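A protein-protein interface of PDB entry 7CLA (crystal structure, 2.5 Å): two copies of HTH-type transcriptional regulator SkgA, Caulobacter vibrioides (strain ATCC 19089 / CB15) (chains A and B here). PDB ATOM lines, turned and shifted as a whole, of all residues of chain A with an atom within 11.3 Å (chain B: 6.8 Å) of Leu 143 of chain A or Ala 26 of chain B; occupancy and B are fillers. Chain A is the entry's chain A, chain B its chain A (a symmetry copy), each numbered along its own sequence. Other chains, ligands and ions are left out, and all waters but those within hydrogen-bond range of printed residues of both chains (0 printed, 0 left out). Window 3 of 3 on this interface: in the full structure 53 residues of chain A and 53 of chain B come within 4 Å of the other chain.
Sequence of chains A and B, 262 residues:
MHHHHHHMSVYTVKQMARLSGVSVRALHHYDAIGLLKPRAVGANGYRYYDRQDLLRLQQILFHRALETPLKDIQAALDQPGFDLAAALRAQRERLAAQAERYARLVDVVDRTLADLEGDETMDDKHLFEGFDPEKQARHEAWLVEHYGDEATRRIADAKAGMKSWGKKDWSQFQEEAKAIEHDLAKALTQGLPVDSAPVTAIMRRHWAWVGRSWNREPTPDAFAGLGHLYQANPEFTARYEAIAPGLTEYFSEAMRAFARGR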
ATOM      1  N   PRO A 133     -25.067  16.017  -0.706  1.00  0.00           N
ATOM      2  CA  PRO A 133     -24.970  16.144   0.743  1.00  0.00           C
ATOM      3  C   PRO A 133     -23.604  16.651   1.213  1.00  0.00           C
ATOM      4  O   PRO A 133     -23.531  17.253   2.298  1.00  0.00           O
ATOM      5  CB  PRO A 133     -25.219  14.711   1.238  1.00  0.00           C
ATOM      6  CG  PRO A 133     -25.910  14.030   0.091  1.00  0.00           C
ATOM      7  CD  PRO A 133     -25.257  14.625  -1.137  1.00  0.00           C
ATOM      8  N   GLU A 134     -22.585  16.357   0.420  1.00  0.00           N
ATOM      9  CA  GLU A 134     -21.202  16.755   0.729  1.00  0.00           C
ATOM     10  C   GLU A 134     -21.136  18.275   0.698  1.00  0.00           C
ATOM     11  O   GLU A 134     -20.612  18.851   1.633  1.00  0.00           O
ATOM     12  CB  GLU A 134     -20.278  16.163  -0.330  1.00  0.00           C
ATOM     13  CG  GLU A 134     -18.834  16.135   0.108  1.00  0.00           C
ATOM     14  CD  GLU A 134     -18.682  16.233   1.611  1.00  0.00           C
ATOM     15  OE1 GLU A 134     -19.290  15.411   2.314  1.00  0.00           O
ATOM     16  OE2 GLU A 134     -17.968  17.132   2.070  1.00  0.00           O
ATOM     17  N   LYS A 135     -21.666  18.868  -0.365  1.00  0.00           N
ATOM     18  CA  LYS A 135     -21.680  20.341  -0.548  1.00  0.00           C
ATOM     19  C   LYS A 135     -22.512  21.023   0.544  1.00  0.00           C
ATOM     20  O   LYS A 135     -22.291  22.217   0.784  1.00  0.00           O
ATOM     21  CB  LYS A 135     -22.249  20.698  -1.917  1.00  0.00           C
ATOM     22  CG  LYS A 135     -21.339  20.335  -3.072  1.00  0.00           C
ATOM     23  CD  LYS A 135     -21.318  21.351  -4.177  1.00  0.00           C
ATOM     24  CE  LYS A 135     -20.021  21.280  -4.948  1.00  0.00           C
ATOM     25  NZ  LYS A 135     -18.940  20.754  -4.090  1.00  0.00           N
ATOM     26  N   GLN A 136     -23.442  20.288   1.147  1.00  0.00           N
ATOM     27  CA  GLN A 136     -24.280  20.847   2.227  1.00  0.00           C
ATOM     28  C   GLN A 136     -23.469  20.811   3.519  1.00  0.00           C
ATOM     29  O   GLN A 136     -23.465  21.796   4.236  1.00  0.00           O
ATOM     30  CB  GLN A 136     -25.570  20.043   2.342  1.00  0.00           C
ATOM     31  CG  GLN A 136     -26.568  20.661   3.294  1.00  0.00           C
ATOM     32  CD  GLN A 136     -27.092  21.916   2.665  1.00  0.00           C
ATOM     33  OE1 GLN A 136     -27.445  21.905   1.504  1.00  0.00           O
ATOM     34  NE2 GLN A 136     -27.094  23.008   3.407  1.00  0.00           N
ATOM     35  N   ALA A 137     -22.772  19.712   3.778  1.00  0.00           N
ATOM     36  CA  ALA A 137     -21.965  19.626   5.009  1.00  0.00           C
ATOM     37  C   ALA A 137     -20.900  20.727   5.020  1.00  0.00           C
ATOM     38  O   ALA A 137     -20.743  21.369   6.061  1.00  0.00           O
ATOM     39  CB  ALA A 137     -21.352  18.265   5.104  1.00  0.00           C
ATOM     40  N   ARG A 138     -20.212  20.933   3.899  1.00  0.00           N
ATOM     41  CA  ARG A 138     -19.132  21.945   3.800  1.00  0.00           C
ATOM     42  C   ARG A 138     -19.702  23.346   3.969  1.00  0.00           C
ATOM     43  O   ARG A 138     -18.918  24.261   4.114  1.00  0.00           O
ATOM     44  CB  ARG A 138     -18.499  21.922   2.409  1.00  0.00           C
ATOM     45  CG  ARG A 138     -17.743  20.649   2.082  1.00  0.00           C
ATOM     46  CD  ARG A 138     -16.974  20.820   0.797  1.00  0.00           C
ATOM     47  NE  ARG A 138     -17.408  19.826  -0.164  1.00  0.00           N
ATOM     48  CZ  ARG A 138     -16.595  19.171  -0.966  1.00  0.00           C
ATOM     49  NH1 ARG A 138     -15.298  19.410  -0.922  1.00  0.00           N
ATOM     50  NH2 ARG A 138     -17.074  18.278  -1.808  1.00  0.00           N
ATOM     51  N   HIS A 139     -21.016  23.489   3.889  1.00  0.00           N
ATOM     52  CA  HIS A 139     -21.669  24.815   4.003  1.00  0.00           C
ATOM     53  C   HIS A 139     -22.241  24.981   5.402  1.00  0.00           C
ATOM     54  O   HIS A 139     -22.190  26.082   5.932  1.00  0.00           O
ATOM     55  CB  HIS A 139     -22.799  24.929   2.986  1.00  0.00           C
ATOM     56  CG  HIS A 139     -23.594  26.177   3.096  1.00  0.00           C
ATOM     57  ND1 HIS A 139     -23.111  27.384   2.691  1.00  0.00           N
ATOM     58  CD2 HIS A 139     -24.848  26.400   3.525  1.00  0.00           C
ATOM     59  CE1 HIS A 139     -24.030  28.298   2.866  1.00  0.00           C
ATOM     60  NE2 HIS A 139     -25.097  27.724   3.371  1.00  0.00           N
ATOM     61  N   GLU A 140     -22.749  23.905   5.964  1.00  0.00           N
ATOM     62  CA  GLU A 140     -23.208  23.993   7.356  1.00  0.00           C
ATOM     63  C   GLU A 140     -21.987  24.162   8.248  1.00  0.00           C
ATOM     64  O   GLU A 140     -22.035  24.973   9.156  1.00  0.00           O
ATOM     65  CB  GLU A 140     -24.135  22.812   7.613  1.00  0.00           C
ATOM     66  CG  GLU A 140     -25.286  22.950   6.648  1.00  0.00           C
ATOM     67  CD  GLU A 140     -26.274  21.836   6.441  1.00  0.00           C
ATOM     68  OE1 GLU A 140     -25.921  20.686   6.626  1.00  0.00           O
ATOM     69  OE2 GLU A 140     -27.365  22.136   6.026  1.00  0.00           O
ATOM     70  N   ALA A 141     -20.903  23.480   7.911  1.00  0.00           N
ATOM     71  CA  ALA A 141     -19.641  23.630   8.673  1.00  0.00           C
ATOM     72  C   ALA A 141     -19.120  25.065   8.635  1.00  0.00           C
ATOM     73  O   ALA A 141     -18.522  25.492   9.610  1.00  0.00           O
ATOM     74  CB  ALA A 141     -18.617  22.696   8.106  1.00  0.00           C
ATOM     75  N   TRP A 142     -19.297  25.738   7.508  1.00  0.00           N
ATOM     76  CA  TRP A 142     -18.878  27.137   7.284  1.00  0.00           C
ATOM     77  C   TRP A 142     -19.741  28.083   8.113  1.00  0.00           C
ATOM     78  O   TRP A 142     -19.226  29.091   8.591  1.00  0.00           O
ATOM     79  CB  TRP A 142     -19.036  27.429   5.797  1.00  0.00           C
ATOM     80  CG  TRP A 142     -18.684  28.826   5.408  1.00  0.00           C
ATOM     81  CD1 TRP A 142     -17.456  29.285   5.043  1.00  0.00           C
ATOM     82  CD2 TRP A 142     -19.575  29.948   5.334  1.00  0.00           C
ATOM     83  NE1 TRP A 142     -17.522  30.615   4.757  1.00  0.00           N
ATOM     84  CE2 TRP A 142     -18.808  31.050   4.921  1.00  0.00           C
ATOM     85  CE3 TRP A 142     -20.936  30.132   5.584  1.00  0.00           C
ATOM     86  CZ2 TRP A 142     -19.363  32.311   4.740  1.00  0.00           C
ATOM     87  CZ3 TRP A 142     -21.485  31.378   5.408  1.00  0.00           C
ATOM     88  CH2 TRP A 142     -20.705  32.451   4.993  1.00  0.00           C
ATOM     89  N   LEU A 143     -21.018  27.749   8.263  1.00  0.00           N
ATOM     90  CA  LEU A 143     -21.981  28.621   8.997  1.00  0.00           C
ATOM     91  C   LEU A 143     -21.689  28.626  10.496  1.00  0.00           C
ATOM     92  O   LEU A 143     -22.090  29.609  11.139  1.00  0.00           O
ATOM     93  CB  LEU A 143     -23.411  28.162   8.726  1.00  0.00           C
ATOM     94  CG  LEU A 143     -23.931  28.511   7.335  1.00  0.00           C
ATOM     95  CD1 LEU A 143     -25.065  27.584   6.950  1.00  0.00           C
ATOM     96  CD2 LEU A 143     -24.362  29.972   7.258  1.00  0.00           C
ATOM     97  N   VAL A 144     -20.965  27.629  11.013  1.00  0.00           N
ATOM     98  CA  VAL A 144     -20.496  27.618  12.433  1.00  0.00           C
ATOM     99  C   VAL A 144     -19.277  28.548  12.564  1.00  0.00           C
ATOM    100  O   VAL A 144     -18.805  28.743  13.699  1.00  0.00           O
ATOM    101  CB  VAL A 144     -20.181  26.190  12.923  1.00  0.00           C
ATOM    102  CG1 VAL A 144     -20.330  26.064  14.432  1.00  0.00           C
ATOM    103  CG2 VAL A 144     -21.040  25.149  12.221  1.00  0.00           C
ATOM    104  N   GLU A 145     -18.801  29.108  11.444  1.00  0.00           N
ATOM    105  CA  GLU A 145     -17.597  29.979  11.339  1.00  0.00           C
ATOM    106  C   GLU A 145     -16.391  29.267  11.960  1.00  0.00           C
ATOM    107  O   GLU A 145     -16.144  28.149  11.553  1.00  0.00           O
ATOM    108  CB  GLU A 145     -17.801  31.328  12.019  1.00  0.00           C
ATOM    109  CG  GLU A 145     -18.757  32.230  11.285  1.00  0.00           C
ATOM    110  CD  GLU A 145     -20.006  32.540  12.096  1.00  0.00           C
ATOM    111  OE1 GLU A 145     -20.605  31.584  12.726  1.00  0.00           O
ATOM    112  OE2 GLU A 145     -20.398  33.732  12.099  1.00  0.00           O
ATOM    113  N   VAL B  22     -31.030  19.863   4.671  1.00  0.00           N
ATOM    114  CA  VAL B  22     -30.327  21.038   5.256  1.00  0.00           C
ATOM    115  C   VAL B  22     -30.382  20.869   6.786  1.00  0.00           C
ATOM    116  O   VAL B  22     -31.347  20.317   7.335  1.00  0.00           O
ATOM    117  CB  VAL B  22     -30.978  22.328   4.753  1.00  0.00           C
ATOM    118  CG1 VAL B  22     -30.362  23.583   5.341  1.00  0.00           C
ATOM    119  CG2 VAL B  22     -30.951  22.411   3.231  1.00  0.00           C
ATOM    120  N   SER B  23     -29.354  21.256   7.510  1.00  0.00           N
ATOM    121  CA  SER B  23     -29.324  20.992   8.960  1.00  0.00           C
ATOM    122  C   SER B  23     -30.186  22.045   9.666  1.00  0.00           C
ATOM    123  O   SER B  23     -30.403  23.161   9.127  1.00  0.00           O
ATOM    124  CB  SER B  23     -27.915  20.967   9.477  1.00  0.00           C
ATOM    125  OG  SER B  23     -27.391  22.309   9.554  1.00  0.00           O
ATOM    126  N   VAL B  24     -30.610  21.710  10.866  1.00  0.00           N
ATOM    127  CA  VAL B  24     -31.214  22.652  11.841  1.00  0.00           C
ATOM    128  C   VAL B  24     -30.320  23.890  12.044  1.00  0.00           C
ATOM    129  O   VAL B  24     -30.870  24.996  11.995  1.00  0.00           O
ATOM    130  CB  VAL B  24     -31.498  21.866  13.122  1.00  0.00           C
ATOM    131  CG1 VAL B  24     -31.913  22.762  14.274  1.00  0.00           C
ATOM    132  CG2 VAL B  24     -32.578  20.801  12.828  1.00  0.00           C
ATOM    133  N   ARG B  25     -28.996  23.718  12.115  1.00  0.00           N
ATOM    134  CA  ARG B  25     -28.002  24.820  12.236  1.00  0.00           C
ATOM    135  C   ARG B  25     -28.200  25.772  11.055  1.00  0.00           C
ATOM    136  O   ARG B  25     -28.504  26.959  11.267  1.00  0.00           O
ATOM    137  CB  ARG B  25     -26.560  24.299  12.332  1.00  0.00           C
ATOM    138  N   ALA B  26     -28.101  25.270   9.838  1.00  0.00           N
ATOM    139  CA  ALA B  26     -28.249  26.144   8.659  1.00  0.00           C
ATOM    140  C   ALA B  26     -29.632  26.825   8.639  1.00  0.00           C
ATOM    141  O   ALA B  26     -29.738  27.991   8.298  1.00  0.00           O
ATOM    142  CB  ALA B  26     -27.969  25.352   7.406  1.00  0.00           C
ATOM    143  N   LEU B  27     -30.704  26.142   8.977  1.00  0.00           N
ATOM    144  CA  LEU B  27     -32.056  26.740   8.792  1.00  0.00           C
ATOM    145  C   LEU B  27     -32.266  27.901   9.770  1.00  0.00           C
ATOM    146  O   LEU B  27     -32.989  28.849   9.441  1.00  0.00           O
ATOM    147  CB  LEU B  27     -33.128  25.647   8.959  1.00  0.00           C
ATOM    148  CG  LEU B  27     -33.149  24.661   7.806  1.00  0.00           C
ATOM    149  CD1 LEU B  27     -34.009  23.476   8.162  1.00  0.00           C
ATOM    150  CD2 LEU B  27     -33.649  25.350   6.535  1.00  0.00           C
ATOM    151  N   HIS B  28     -31.673  27.795  10.942  1.00  0.00           N
ATOM    152  CA  HIS B  28     -31.710  28.852  11.984  1.00  0.00           C
ATOM    153  C   HIS B  28     -30.893  30.058  11.518  1.00  0.00           C
ATOM    154  O   HIS B  28     -31.336  31.200  11.717  1.00  0.00           O
ATOM    155  CB  HIS B  28     -31.167  28.298  13.295  1.00  0.00           C
ATOM    156  CG  HIS B  28     -32.177  27.514  14.053  1.00  0.00           C
ATOM    157  ND1 HIS B  28     -31.869  26.322  14.641  1.00  0.00           N
ATOM    158  CD2 HIS B  28     -33.470  27.774  14.341  1.00  0.00           C
ATOM    159  CE1 HIS B  28     -32.935  25.877  15.289  1.00  0.00           C
ATOM    160  NE2 HIS B  28     -33.953  26.733  15.099  1.00  0.00           N
ATOM    161  N   HIS B  29     -29.786  29.796  10.828  1.00  0.00           N
ATOM    162  CA  HIS B  29     -28.936  30.848  10.241  1.00  0.00           C
ATOM    163  C   HIS B  29     -29.656  31.523   9.083  1.00  0.00           C
ATOM    164  O   HIS B  29     -29.723  32.794   9.088  1.00  0.00           O
ATOM    165  CB  HIS B  29     -27.540  30.285  10.021  1.00  0.00           C
ATOM    166  CG  HIS B  29     -26.852  30.125  11.353  1.00  0.00           C
ATOM    167  ND1 HIS B  29     -27.026  31.051  12.426  1.00  0.00           N
ATOM    168  CD2 HIS B  29     -26.055  29.144  11.842  1.00  0.00           C
ATOM    169  CE1 HIS B  29     -26.323  30.651  13.457  1.00  0.00           C
ATOM    170  NE2 HIS B  29     -25.707  29.490  13.125  1.00  0.00           N
ATOM    171  N   TYR B  30     -30.281  30.726   8.218  1.00  0.00           N
ATOM    172  CA  TYR B  30     -31.044  31.236   7.058  1.00  0.00           C
ATOM    173  C   TYR B  30     -32.179  32.085   7.579  1.00  0.00           C
ATOM    174  O   TYR B  30     -32.510  33.085   6.948  1.00  0.00           O
ATOM    175  CB  TYR B  30     -31.584  30.119   6.184  1.00  0.00           C
ATOM    176  CG  TYR B  30     -30.570  29.401   5.333  1.00  0.00           C
ATOM    177  CD1 TYR B  30     -29.223  29.701   5.357  1.00  0.00           C
ATOM    178  CD2 TYR B  30     -30.981  28.376   4.495  1.00  0.00           C
ATOM    179  CE1 TYR B  30     -28.321  29.006   4.562  1.00  0.00           C
ATOM    180  CE2 TYR B  30     -30.095  27.687   3.684  1.00  0.00           C
ATOM    181  CZ  TYR B  30     -28.756  28.003   3.714  1.00  0.00           C
ATOM    182  OH  TYR B  30     -27.899  27.274   2.947  1.00  0.00           O
ATOM    183  N   ASP B  31     -32.745  31.691   8.712  1.00  0.00           N
ATOM    184  CA  ASP B  31     -33.864  32.431   9.375  1.00  0.00           C
ATOM    185  C   ASP B  31     -33.350  33.762   9.940  1.00  0.00           C
ATOM    186  O   ASP B  31     -34.012  34.789   9.778  1.00  0.00           O
ATOM    187  CB  ASP B  31     -34.490  31.580  10.480  1.00  0.00           C
ATOM    188  CG  ASP B  31     -35.742  32.149  11.133  1.00  0.00           C
ATOM    189  OD1 ASP B  31     -36.369  33.086  10.610  1.00  0.00           O
ATOM    190  OD2 ASP B  31     -36.110  31.610  12.167  1.00  0.00           O
ATOM    191  N   ALA B  32     -32.221  33.730  10.625  1.00  0.00           N
ATOM    192  CA  ALA B  32     -31.695  34.899  11.355  1.00  0.00           C
ATOM    193  C   ALA B  32     -31.390  36.004  10.326  1.00  0.00           C
ATOM    194  O   ALA B  32     -31.813  37.184  10.551  1.00  0.00           O
ATOM    195  CB  ALA B  32     -30.491  34.500  12.173  1.00  0.00           C
ATOM    196  N   ILE B  33     -30.783  35.620   9.192  1.00  0.00           N
ATOM    197  CA  ILE B  33     -30.288  36.592   8.164  1.00  0.00           C
ATOM    198  C   ILE B  33     -31.397  36.952   7.152  1.00  0.00           C
ATOM    199  O   ILE B  33     -31.095  37.689   6.198  1.00  0.00           O
ATOM    200  CB  ILE B  33     -29.019  36.086   7.460  1.00  0.00           C
ATOM    201  CG1 ILE B  33     -29.348  35.089   6.342  1.00  0.00           C
ATOM    202  CG2 ILE B  33     -28.018  35.534   8.468  1.00  0.00           C
ATOM    203  CD1 ILE B  33     -28.160  34.339   5.798  1.00  0.00           C
ATOM    204  N   ARG B  64     -26.980  27.255  -4.695  1.00  0.00           N
ATOM    205  CA  ARG B  64     -25.731  26.709  -4.130  1.00  0.00           C
ATOM    206  C   ARG B  64     -25.147  25.633  -5.038  1.00  0.00           C
ATOM    207  O   ARG B  64     -23.955  25.481  -5.032  1.00  0.00           O
ATOM    208  CB  ARG B  64     -25.962  26.305  -2.678  1.00  0.00           C
ATOM    209  CG  ARG B  64     -26.197  27.516  -1.797  1.00  0.00           C
ATOM    210  CD  ARG B  64     -26.269  27.138  -0.350  1.00  0.00           C
ATOM    211  NE  ARG B  64     -25.158  26.250  -0.108  1.00  0.00           N
ATOM    212  CZ  ARG B  64     -25.255  25.070   0.472  1.00  0.00           C
ATOM    213  NH1 ARG B  64     -26.428  24.627   0.885  1.00  0.00           N
ATOM    214  NH2 ARG B  64     -24.172  24.342   0.646  1.00  0.00           N
ATOM    215  N   LEU B  70     -23.948  33.340  -1.045  1.00  0.00           N
ATOM    216  CA  LEU B  70     -25.061  33.510  -0.094  1.00  0.00           C
ATOM    217  C   LEU B  70     -25.713  34.896  -0.203  1.00  0.00           C
ATOM    218  O   LEU B  70     -26.954  34.940  -0.320  1.00  0.00           O
ATOM    219  CB  LEU B  70     -24.539  33.226   1.309  1.00  0.00           C
ATOM    220  CG  LEU B  70     -25.604  32.873   2.354  1.00  0.00           C
ATOM    221  CD1 LEU B  70     -26.784  32.092   1.756  1.00  0.00           C
ATOM    222  CD2 LEU B  70     -24.980  32.083   3.506  1.00  0.00           C
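OH of Tyr 30 of chain B is in hydrogen-bond range of NE2 of His 139 of chain A (2.9 Å).
NH1 of Arg 64 of chain B sits at hydrogen-bond distance from OE1 of Gln 136 of chain A (3.0 Å).
The side-chain carboxylate (OE2) of Glu 140 of chain A lies within hydrogen-bond range of the backbone NH (N) of Ser 23 of chain B, 2.6 Å away.
The backbone carbonyl oxygen (O) of Lys 135 of chain A sits at hydrogen-bond distance from the guanidinium group (NH2) of Arg 64 of chain B (2.8 Å).
The backbone NH (N) of Arg 25 of chain B sits close to the side-chain hydroxyl (OG) of Ser 23 of chain B (3.3 Å).
The side-chain amide nitrogen (NE2) of Gln 136 of chain A lies within hydrogen-bond range of the side-chain carboxylate (OE2) of Glu 140 of chain A (2.8 Å).
OG of Ser 23 of chain B lies within hydrogen-bond range of N of Ala 26 of chain B, at 3.1 Å.
CG1 of Val 22 of chain B touches NE2 of Gln 136 of chain A, at 3.8 Å.
His 139 of chain A touches Arg 64 of chain B.
His 139 of chain A touches Leu 70 of chain B.
OE2 of Glu 140 of chain A touches CA of Val 22 of chain B, at 3.3 Å.
CB of Ala 26 of chain B touches OE2 of Glu 140 of chain A, at 3.6 Å.
Leu 143 of chain A touches Ala 26 of chain B (CD1 to CB, 3.7 Å).
Printed residues of chain B within 4 Å of Lys 135 of chain A: Arg 64 (2.8 Å).
Printed residues of chain B within 4 Å of Gln 136 of chain A: Val 22 (3.8 Å) and Arg 64 (3.0 Å).
Of the printed residues of chain B, His 139 of chain A touches Tyr 30 (2.9 Å), Arg 64 (2.8 Å) and Leu 70 (3.95 Å).
Of the printed residues of chain B, Glu 140 of chain A touches Val 22 (3.3 Å), Ser 23 (2.6 Å) and Ala 26 (3.6 Å).
Leu 143 of chain A touches just one residue of chain B: Ala 26 (3.7 Å).
Of chain A, only Gln 136 and Glu 140 come within 4 Å of Val 22 of chain B.
Of the printed residues of chain A, Ser 23 of chain B touches Glu 140.
No residue of chain A comes within 4 Å of Val 24 of chain B.
No residue of chain A comes within 4 Å of Arg 25 of chain B.
Ala 26 of chain B touches just these residues of chain A: Glu 140 and Leu 143.
No residue of chain A comes within 4 Å of His 29 of chain B.
Of the printed residues of chain A, Leu 70 of chain B touches His 139 (3.95 Å).
The nearest residue of chain B that does not touch Leu 143 of chain A is His 29 of chain B (4.1 Å).
The nearest residue of chain A that does not touch Ala 26 of chain B is Gln 136 of chain A (4.7 Å).
Of the 14 printed residues of chain B, 6 touch a printed residue of chain A.
Hydrophobic or aromatic side chains of chain B that line the printed part of chain A: Val 22, Ala 26, Tyr 30 and Leu 70.
Printed residues of chain A that touch a printed residue of chain B: Lys 135, Gln 136, His 139, Glu 140 and Leu 143.
Hydrophobic or aromatic side chains of chain A within 4 Å of the printed part of chain B: His 139 and Leu 143.
Among the printed residues, 10 pairs touch across the chains.
Among the printed residues, no Asp or Glu carboxylate lies within 4 Å of a Lys or Arg side-chain nitrogen of the other chain.
No position is printed for both chains.
Of the 10 pairs that touch across the chains among the printed residues, none has its exchanged pair printed and touching as well.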
